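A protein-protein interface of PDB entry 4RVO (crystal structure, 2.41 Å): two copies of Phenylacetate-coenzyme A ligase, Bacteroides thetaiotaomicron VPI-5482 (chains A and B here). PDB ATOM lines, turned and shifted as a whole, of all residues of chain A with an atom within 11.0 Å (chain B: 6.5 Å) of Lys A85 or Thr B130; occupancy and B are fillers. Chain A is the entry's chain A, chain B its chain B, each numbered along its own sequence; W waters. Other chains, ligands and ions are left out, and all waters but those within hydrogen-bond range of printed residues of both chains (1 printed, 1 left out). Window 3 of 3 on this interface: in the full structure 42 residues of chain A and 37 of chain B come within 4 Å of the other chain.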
ATOM      1  N   PHE A  77      10.512  29.412  -3.771  1.00  0.00           N
ATOM      2  CA  PHE A  77       9.329  29.419  -4.634  1.00  0.00           C
ATOM      3  C   PHE A  77       9.548  30.208  -5.962  1.00  0.00           C
ATOM      4  O   PHE A  77       8.577  30.586  -6.613  1.00  0.00           O
ATOM      5  CB  PHE A  77       8.127  29.997  -3.877  1.00  0.00           C
ATOM      6  CG  PHE A  77       7.886  29.361  -2.519  1.00  0.00           C
ATOM      7  CD1 PHE A  77       7.648  27.993  -2.406  1.00  0.00           C
ATOM      8  CD2 PHE A  77       7.795  30.143  -1.372  1.00  0.00           C
ATOM      9  CE1 PHE A  77       7.391  27.415  -1.159  1.00  0.00           C
ATOM     10  CE2 PHE A  77       7.538  29.561  -0.128  1.00  0.00           C
ATOM     11  CZ  PHE A  77       7.330  28.203  -0.032  1.00  0.00           C
ATOM     12  N   VAL A  80       7.560  28.579  -8.821  1.00  0.00           N
ATOM     13  CA  VAL A  80       6.111  28.399  -8.616  1.00  0.00           C
ATOM     14  C   VAL A  80       5.332  29.257  -9.641  1.00  0.00           C
ATOM     15  O   VAL A  80       5.545  30.472  -9.722  1.00  0.00           O
ATOM     16  CB  VAL A  80       5.683  28.725  -7.155  1.00  0.00           C
ATOM     17  CG1 VAL A  80       4.155  28.765  -7.024  1.00  0.00           C
ATOM     18  CG2 VAL A  80       6.285  27.724  -6.178  1.00  0.00           C
ATOM     19  N   ALA A  81       4.453  28.611 -10.434  1.00  0.00           N
ATOM     20  CA  ALA A  81       3.733  29.281 -11.515  1.00  0.00           C
ATOM     21  C   ALA A  81       2.266  29.575 -11.137  1.00  0.00           C
ATOM     22  O   ALA A  81       1.683  30.539 -11.639  1.00  0.00           O
ATOM     23  CB  ALA A  81       3.782  28.433 -12.770  1.00  0.00           C
ATOM     24  N   GLY A  82       1.675  28.712 -10.305  1.00  0.00           N
ATOM     25  CA  GLY A  82       0.273  28.835  -9.914  1.00  0.00           C
ATOM     26  C   GLY A  82       0.046  29.716  -8.703  1.00  0.00           C
ATOM     27  O   GLY A  82       0.989  30.340  -8.195  1.00  0.00           O
ATOM     28  N   ASP A  83      -1.230  29.803  -8.241  1.00  0.00           N
ATOM     29  CA  ASP A  83      -1.581  30.576  -7.048  1.00  0.00           C
ATOM     30  C   ASP A  83      -1.388  29.717  -5.800  1.00  0.00           C
ATOM     31  O   ASP A  83      -2.291  28.964  -5.407  1.00  0.00           O
ATOM     32  CB  ASP A  83      -3.033  31.098  -7.139  1.00  0.00           C
ATOM     33  CG  ASP A  83      -3.395  32.121  -6.062  1.00  0.00           C
ATOM     34  OD1 ASP A  83      -2.674  32.187  -5.029  1.00  0.00           O
ATOM     35  OD2 ASP A  83      -4.401  32.834  -6.241  1.00  0.00           O
ATOM     36  N   MET A  84      -0.210  29.808  -5.198  1.00  0.00           N
ATOM     37  CA  MET A  84       0.187  28.970  -4.074  1.00  0.00           C
ATOM     38  C   MET A  84      -0.718  29.200  -2.850  1.00  0.00           C
ATOM     39  O   MET A  84      -1.090  28.244  -2.175  1.00  0.00           O
ATOM     40  CB  MET A  84       1.642  29.249  -3.719  1.00  0.00           C
ATOM     41  CG  MET A  84       2.248  28.238  -2.790  1.00  0.00           C
ATOM     42  SD  MET A  84       4.139  28.519  -2.608  1.00  0.00           S
ATOM     43  CE  MET A  84       4.113  30.296  -1.962  1.00  0.00           C
ATOM     44  N   LYS A  85      -1.098  30.454  -2.593  1.00  0.00           N
ATOM     45  CA  LYS A  85      -1.924  30.799  -1.425  1.00  0.00           C
ATOM     46  C   LYS A  85      -3.329  30.161  -1.518  1.00  0.00           C
ATOM     47  O   LYS A  85      -3.857  29.699  -0.516  1.00  0.00           O
ATOM     48  CB  LYS A  85      -2.044  32.323  -1.291  1.00  0.00           C
ATOM     49  CG  LYS A  85      -2.451  32.785   0.098  1.00  0.00           C
ATOM     50  CD  LYS A  85      -2.374  34.294   0.227  1.00  0.00           C
ATOM     51  N   ARG A  86      -3.903  30.107  -2.732  1.00  0.00           N
ATOM     52  CA  ARG A  86      -5.265  29.607  -2.937  1.00  0.00           C
ATOM     53  C   ARG A  86      -5.285  28.107  -3.329  1.00  0.00           C
ATOM     54  O   ARG A  86      -6.209  27.389  -2.941  1.00  0.00           O
ATOM     55  CB  ARG A  86      -5.982  30.440  -4.027  1.00  0.00           C
ATOM     56  CG  ARG A  86      -7.462  30.062  -4.214  1.00  0.00           C
ATOM     57  CD  ARG A  86      -8.124  30.838  -5.346  1.00  0.00           C
ATOM     58  NE  ARG A  86      -7.613  30.441  -6.660  1.00  0.00           N
ATOM     59  CZ  ARG A  86      -7.047  31.285  -7.521  1.00  0.00           C
ATOM     60  NH1 ARG A  86      -6.957  32.578  -7.230  1.00  0.00           N
ATOM     61  NH2 ARG A  86      -6.605  30.848  -8.694  1.00  0.00           N
ATOM     62  N   ASP A  87      -4.324  27.663  -4.171  1.00  0.00           N
ATOM     63  CA  ASP A  87      -4.403  26.344  -4.779  1.00  0.00           C
ATOM     64  C   ASP A  87      -3.288  25.379  -4.278  1.00  0.00           C
ATOM     65  O   ASP A  87      -3.400  24.173  -4.473  1.00  0.00           O
ATOM     66  CB  ASP A  87      -4.351  26.462  -6.305  1.00  0.00           C
ATOM     67  CG  ASP A  87      -5.521  27.251  -6.900  1.00  0.00           C
ATOM     68  OD1 ASP A  87      -6.661  27.057  -6.437  1.00  0.00           O
ATOM     69  OD2 ASP A  87      -5.301  27.980  -7.886  1.00  0.00           O
ATOM     70  N   GLY A  88      -2.251  25.921  -3.637  1.00  0.00           N
ATOM     71  CA  GLY A  88      -1.149  25.104  -3.108  1.00  0.00           C
ATOM     72  C   GLY A  88      -1.563  24.266  -1.915  1.00  0.00           C
ATOM     73  O   GLY A  88      -2.084  24.799  -0.935  1.00  0.00           O
ATOM     74  N   VAL A  89      -1.386  22.930  -2.004  1.00  0.00           N
ATOM     75  CA  VAL A  89      -1.859  22.030  -0.936  1.00  0.00           C
ATOM     76  C   VAL A  89      -0.689  21.179  -0.318  1.00  0.00           C
ATOM     77  O   VAL A  89      -0.894  20.543   0.713  1.00  0.00           O
ATOM     78  CB  VAL A  89      -3.014  21.106  -1.413  1.00  0.00           C
ATOM     79  CG1 VAL A  89      -4.277  21.915  -1.704  1.00  0.00           C
ATOM     80  CG2 VAL A  89      -2.601  20.288  -2.623  1.00  0.00           C
ATOM     81  N   ARG A  90       0.523  21.179  -0.942  1.00  0.00           N
ATOM     82  CA  ARG A  90       1.638  20.422  -0.354  1.00  0.00           C
ATOM     83  C   ARG A  90       3.004  20.907  -0.833  1.00  0.00           C
ATOM     84  O   ARG A  90       3.177  21.214  -2.010  1.00  0.00           O
ATOM     85  CB  ARG A  90       1.508  18.923  -0.650  1.00  0.00           C
ATOM     86  CG  ARG A  90       2.364  18.067   0.295  1.00  0.00           C
ATOM     87  CD  ARG A  90       2.397  16.639  -0.112  1.00  0.00           C
ATOM     88  NE  ARG A  90       1.105  15.992   0.057  1.00  0.00           N
ATOM     89  CZ  ARG A  90       0.834  14.775  -0.386  1.00  0.00           C
ATOM     90  NH1 ARG A  90       1.757  14.080  -1.036  1.00  0.00           N
ATOM     91  NH2 ARG A  90      -0.366  14.251  -0.203  1.00  0.00           N
ATOM     92  N   ILE A  91       4.018  20.815   0.069  1.00  0.00           N
ATOM     93  CA  ILE A  91       5.422  21.065  -0.260  1.00  0.00           C
ATOM     94  C   ILE A  91       6.235  19.813  -0.001  1.00  0.00           C
ATOM     95  O   ILE A  91       6.131  19.221   1.079  1.00  0.00           O
ATOM     96  CB  ILE A  91       5.992  22.264   0.557  1.00  0.00           C
ATOM     97  CG1 ILE A  91       5.218  23.553   0.288  1.00  0.00           C
ATOM     98  CG2 ILE A  91       7.507  22.445   0.296  1.00  0.00           C
ATOM     99  CD1 ILE A  91       5.614  24.715   1.222  1.00  0.00           C
ATOM    100  N   VAL A 105       6.246  22.263  -5.115  1.00  0.00           N
ATOM    101  CA  VAL A 105       4.930  22.630  -4.575  1.00  0.00           C
ATOM    102  C   VAL A 105       3.834  22.032  -5.461  1.00  0.00           C
ATOM    103  O   VAL A 105       3.929  22.103  -6.687  1.00  0.00           O
ATOM    104  CB  VAL A 105       4.768  24.172  -4.430  1.00  0.00           C
ATOM    105  CG1 VAL A 105       3.446  24.520  -3.731  1.00  0.00           C
ATOM    106  CG2 VAL A 105       5.954  24.778  -3.675  1.00  0.00           C
ATOM    107  N   HIS A 106       2.816  21.405  -4.843  1.00  0.00           N
ATOM    108  CA  HIS A 106       1.747  20.739  -5.584  1.00  0.00           C
ATOM    109  C   HIS A 106       0.398  21.390  -5.330  1.00  0.00           C
ATOM    110  O   HIS A 106       0.090  21.753  -4.187  1.00  0.00           O
ATOM    111  CB  HIS A 106       1.671  19.252  -5.200  1.00  0.00           C
ATOM    112  CG  HIS A 106       2.876  18.459  -5.587  1.00  0.00           C
ATOM    113  ND1 HIS A 106       2.923  17.757  -6.778  1.00  0.00           N
ATOM    114  CD2 HIS A 106       4.009  18.215  -4.890  1.00  0.00           C
ATOM    115  CE1 HIS A 106       4.095  17.147  -6.787  1.00  0.00           C
ATOM    116  NE2 HIS A 106       4.784  17.391  -5.671  1.00  0.00           N
ATOM    117  N   SER A 107      -0.462  21.421  -6.367  1.00  0.00           N
ATOM    118  CA  SER A 107      -1.871  21.735  -6.210  1.00  0.00           C
ATOM    119  C   SER A 107      -2.665  20.440  -6.071  1.00  0.00           C
ATOM    120  O   SER A 107      -2.080  19.346  -6.175  1.00  0.00           O
ATOM    121  CB  SER A 107      -2.376  22.551  -7.394  1.00  0.00           C
ATOM    122  OG  SER A 107      -2.308  21.805  -8.599  1.00  0.00           O
ATOM    123  N   GLN A 108      -3.983  20.534  -5.807  1.00  0.00           N
ATOM    124  CA  GLN A 108      -4.809  19.331  -5.661  1.00  0.00           C
ATOM    125  C   GLN A 108      -4.819  18.526  -6.973  1.00  0.00           C
ATOM    126  O   GLN A 108      -4.729  17.299  -6.942  1.00  0.00           O
ATOM    127  CB  GLN A 108      -6.243  19.690  -5.228  1.00  0.00           C
ATOM    128  CG  GLN A 108      -7.100  18.460  -4.887  1.00  0.00           C
ATOM    129  CD  GLN A 108      -6.437  17.582  -3.839  1.00  0.00           C
ATOM    130  OE1 GLN A 108      -5.959  18.058  -2.802  1.00  0.00           O
ATOM    131  NE2 GLN A 108      -6.407  16.282  -4.087  1.00  0.00           N
ATOM    132  N   MET A 295       1.018  23.672 -10.635  1.00  0.00           N
ATOM    133  CA  MET A 295       1.527  24.578  -9.585  1.00  0.00           C
ATOM    134  C   MET A 295       3.005  24.918  -9.831  1.00  0.00           C
ATOM    135  O   MET A 295       3.378  26.096  -9.825  1.00  0.00           O
ATOM    136  CB  MET A 295       1.341  23.956  -8.187  1.00  0.00           C
ATOM    137  CG  MET A 295       1.850  24.859  -7.027  1.00  0.00           C
ATOM    138  SD  MET A 295       1.030  26.640  -6.970  1.00  0.00           S
ATOM    139  CE  MET A 295      -0.763  26.142  -6.812  1.00  0.00           C
ATOM    140  N   ILE B 127      -8.162  28.587  11.117  1.00  0.00           N
ATOM    141  CA  ILE B 127      -7.227  28.208  10.055  1.00  0.00           C
ATOM    142  C   ILE B 127      -7.982  28.136   8.696  1.00  0.00           C
ATOM    143  O   ILE B 127      -9.127  27.673   8.647  1.00  0.00           O
ATOM    144  CB  ILE B 127      -6.496  26.874  10.399  1.00  0.00           C
ATOM    145  CG1 ILE B 127      -5.724  27.002  11.738  1.00  0.00           C
ATOM    146  CG2 ILE B 127      -5.560  26.444   9.258  1.00  0.00           C
ATOM    147  CD1 ILE B 127      -5.168  25.684  12.279  1.00  0.00           C
ATOM    148  N   ARG B 128      -7.384  28.711   7.638  1.00  0.00           N
ATOM    149  CA  ARG B 128      -8.010  28.775   6.311  1.00  0.00           C
ATOM    150  C   ARG B 128      -7.094  28.155   5.253  1.00  0.00           C
ATOM    151  O   ARG B 128      -5.957  27.775   5.565  1.00  0.00           O
ATOM    152  CB  ARG B 128      -8.342  30.237   5.938  1.00  0.00           C
ATOM    153  CG  ARG B 128      -9.277  30.948   6.940  1.00  0.00           C
ATOM    154  CD  ARG B 128     -10.685  30.382   6.903  1.00  0.00           C
ATOM    155  NE  ARG B 128     -11.573  31.075   7.837  1.00  0.00           N
ATOM    156  CZ  ARG B 128     -11.841  30.644   9.067  1.00  0.00           C
ATOM    157  NH1 ARG B 128     -11.323  29.500   9.505  1.00  0.00           N
ATOM    158  NH2 ARG B 128     -12.653  31.332   9.855  1.00  0.00           N
ATOM    159  N   LYS B 129      -7.575  28.065   3.995  1.00  0.00           N
ATOM    160  CA  LYS B 129      -6.783  27.493   2.900  1.00  0.00           C
ATOM    161  C   LYS B 129      -5.540  28.363   2.608  1.00  0.00           C
ATOM    162  O   LYS B 129      -4.576  27.880   2.021  1.00  0.00           O
ATOM    163  CB  LYS B 129      -7.645  27.326   1.622  1.00  0.00           C
ATOM    164  CG  LYS B 129      -8.208  28.651   1.069  1.00  0.00           C
ATOM    165  CD  LYS B 129      -9.115  28.431  -0.162  1.00  0.00           C
ATOM    166  CE  LYS B 129     -10.445  27.811   0.202  1.00  0.00           C
ATOM    167  NZ  LYS B 129     -11.325  27.662  -0.987  1.00  0.00           N
ATOM    168  N   THR B 130      -5.556  29.641   3.064  1.00  0.00           N
ATOM    169  CA  THR B 130      -4.448  30.580   2.840  1.00  0.00           C
ATOM    170  C   THR B 130      -3.300  30.340   3.840  1.00  0.00           C
ATOM    171  O   THR B 130      -2.243  30.968   3.724  1.00  0.00           O
ATOM    172  CB  THR B 130      -4.953  32.024   2.936  1.00  0.00           C
ATOM    173  OG1 THR B 130      -5.560  32.226   4.219  1.00  0.00           O
ATOM    174  CG2 THR B 130      -5.942  32.366   1.831  1.00  0.00           C
ATOM    175  N   ASP B 131      -3.511  29.451   4.824  1.00  0.00           N
ATOM    176  CA  ASP B 131      -2.505  29.183   5.839  1.00  0.00           C
ATOM    177  C   ASP B 131      -1.489  28.141   5.363  1.00  0.00           C
ATOM    178  O   ASP B 131      -1.817  27.271   4.545  1.00  0.00           O
ATOM    179  CB  ASP B 131      -3.167  28.710   7.154  1.00  0.00           C
ATOM    180  CG  ASP B 131      -3.827  29.827   7.934  1.00  0.00           C
ATOM    181  OD1 ASP B 131      -3.097  30.693   8.464  1.00  0.00           O
ATOM    182  OD2 ASP B 131      -5.064  29.811   8.054  1.00  0.00           O
ATOM    183  N   VAL B 132      -0.263  28.217   5.896  1.00  0.00           N
ATOM    184  CA  VAL B 132       0.761  27.218   5.659  1.00  0.00           C
ATOM    185  C   VAL B 132       0.830  26.292   6.886  1.00  0.00           C
ATOM    186  O   VAL B 132       1.239  26.732   7.965  1.00  0.00           O
ATOM    187  CB  VAL B 132       2.139  27.874   5.344  1.00  0.00           C
ATOM    188  CG1 VAL B 132       3.190  26.815   5.014  1.00  0.00           C
ATOM    189  CG2 VAL B 132       2.014  28.888   4.207  1.00  0.00           C
ATOM    190  N   GLY B 156      -7.518  22.894   2.397  1.00  0.00           N
ATOM    191  CA  GLY B 156      -6.830  23.551   1.288  1.00  0.00           C
ATOM    192  C   GLY B 156      -5.544  24.250   1.681  1.00  0.00           C
ATOM    193  O   GLY B 156      -4.980  25.004   0.883  1.00  0.00           O
ATOM    194  N   CYS B 157      -5.050  23.988   2.916  1.00  0.00           N
ATOM    195  CA  CYS B 157      -3.798  24.586   3.412  1.00  0.00           C
ATOM    196  C   CYS B 157      -2.623  24.146   2.564  1.00  0.00           C
ATOM    197  O   CYS B 157      -2.598  23.009   2.077  1.00  0.00           O
ATOM    198  CB  CYS B 157      -3.569  24.225   4.880  1.00  0.00           C
ATOM    199  SG  CYS B 157      -4.879  24.763   5.990  1.00  0.00           S
ATOM    200  N   LEU B 158      -1.582  24.981   2.505  1.00  0.00           N
ATOM    201  CA  LEU B 158      -0.301  24.574   1.975  1.00  0.00           C
ATOM    202  C   LEU B 158       0.419  23.748   3.031  1.00  0.00           C
ATOM    203  O   LEU B 158       0.874  24.304   4.033  1.00  0.00           O
ATOM    204  CB  LEU B 158       0.528  25.813   1.573  1.00  0.00           C
ATOM    205  CG  LEU B 158       1.880  25.536   0.939  1.00  0.00           C
ATOM    206  CD1 LEU B 158       1.722  24.778  -0.368  1.00  0.00           C
ATOM    207  CD2 LEU B 158       2.639  26.818   0.715  1.00  0.00           C
ATOM    208  N   THR B 180       2.268  29.303   9.123  1.00  0.00           N
ATOM    209  CA  THR B 180       1.373  30.106   9.971  1.00  0.00           C
ATOM    210  C   THR B 180       0.665  29.220  11.003  1.00  0.00           C
ATOM    211  O   THR B 180       0.283  29.705  12.072  1.00  0.00           O
ATOM    212  CB  THR B 180       0.356  30.864   9.108  1.00  0.00           C
ATOM    213  OG1 THR B 180      -0.396  29.924   8.342  1.00  0.00           O
ATOM    214  CG2 THR B 180       1.017  31.873   8.185  1.00  0.00           C
HETATM  215  O   HOH W   1      -5.707  25.221  -1.544  1.00  0.00           O
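Among the printed residues, merely in contact across the chains: Lys A85 with Thr B130 (3.5 Å), Gly A88 with Cys B157 (3.5 Å), Ile A91 with Leu B158 (3.7 Å), Val A105 with Leu B158 (3.8 Å), Met A84 with Leu B158 (3.8 Å), Arg A90 with Leu B158 (3.8 Å) and Val A89 with Leu B158 (3.97 Å).
Ala A81 touches none of the printed residues of chain B.
Printed residues of chain B within 4 Å of Arg A90: Leu B158.
Of the printed residues of chain B, Ile A91 touches Leu B158 (3.7 Å).
Of the printed residues of chain B, Val A105 touches Leu B158 (3.8 Å).
Thr B130 touches just one residue of chain A: Lys A85.
No residue of chain A comes within 4 Å of Asp B131.
Val B132 touches none of the printed residues of chain A.
Printed residues of chain A within 4 Å of Cys B157: Gly A88 (3.5 Å) and Val A89 (3.3 Å).
The nearest residue of chain A that does not touch Thr B130 is Arg A86 (5.5 Å).
No position is printed for both chains.
Water W1 lies within hydrogen-bond range of the backbone carbonyl oxygen (O) of Gly B156 (2.5 Å) and the backbone carbonyl oxygen (O) of Arg A86 (2.6 Å).
The backbone carbonyl oxygen of Val A89 sits close to the backbone carbonyl oxygen of Cys B157, 3.3 Å away.
The backbone NH of Leu B158 lies close to the backbone carbonyl oxygen of Gly A88 (3.5 Å).
The backbone carbonyl oxygen (O) of Lys A85 lies close to the backbone carbonyl oxygen (O) of Lys B129, 3.2 Å away.
O of Gly B156 sits close to O of Gly A88.
Printed residues of chain A that touch a printed residue of chain B: Met A84, Lys A85, Gly A88, Val A89, Arg A90, Ile A91 and Val A105.
Hydrophobic or aromatic side chains of chain A within 4 Å of the printed part of chain B: Met A84, Val A89, Ile A91 and Val A105.
Of the 10 printed residues of chain B, 5 touch a printed residue of chain A.
Hydrophobic or aromatic side chains of chain B within 4 Å of the printed part of chain A: Leu B158.
Among the printed residues, 11 pairs touch across the chains.
O of Asp B131 lies within hydrogen-bond range of N of Leu B158 (3.1 Å).
O of His A106 sits at hydrogen-bond distance from N of Val A89, at 2.9 Å.
The backbone carbonyl oxygen of Arg A90 sits at hydrogen-bond distance from the backbone NH of His A106 (2.9 Å).
The backbone carbonyl oxygen (O) of Arg B128 lies within hydrogen-bond range of the side-chain sulfur (SG) of Cys B157, at 3.2 Å.
The side-chain carboxylate of Asp A83 lies close to the backbone NH of Lys A85, 3.4 Å away.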
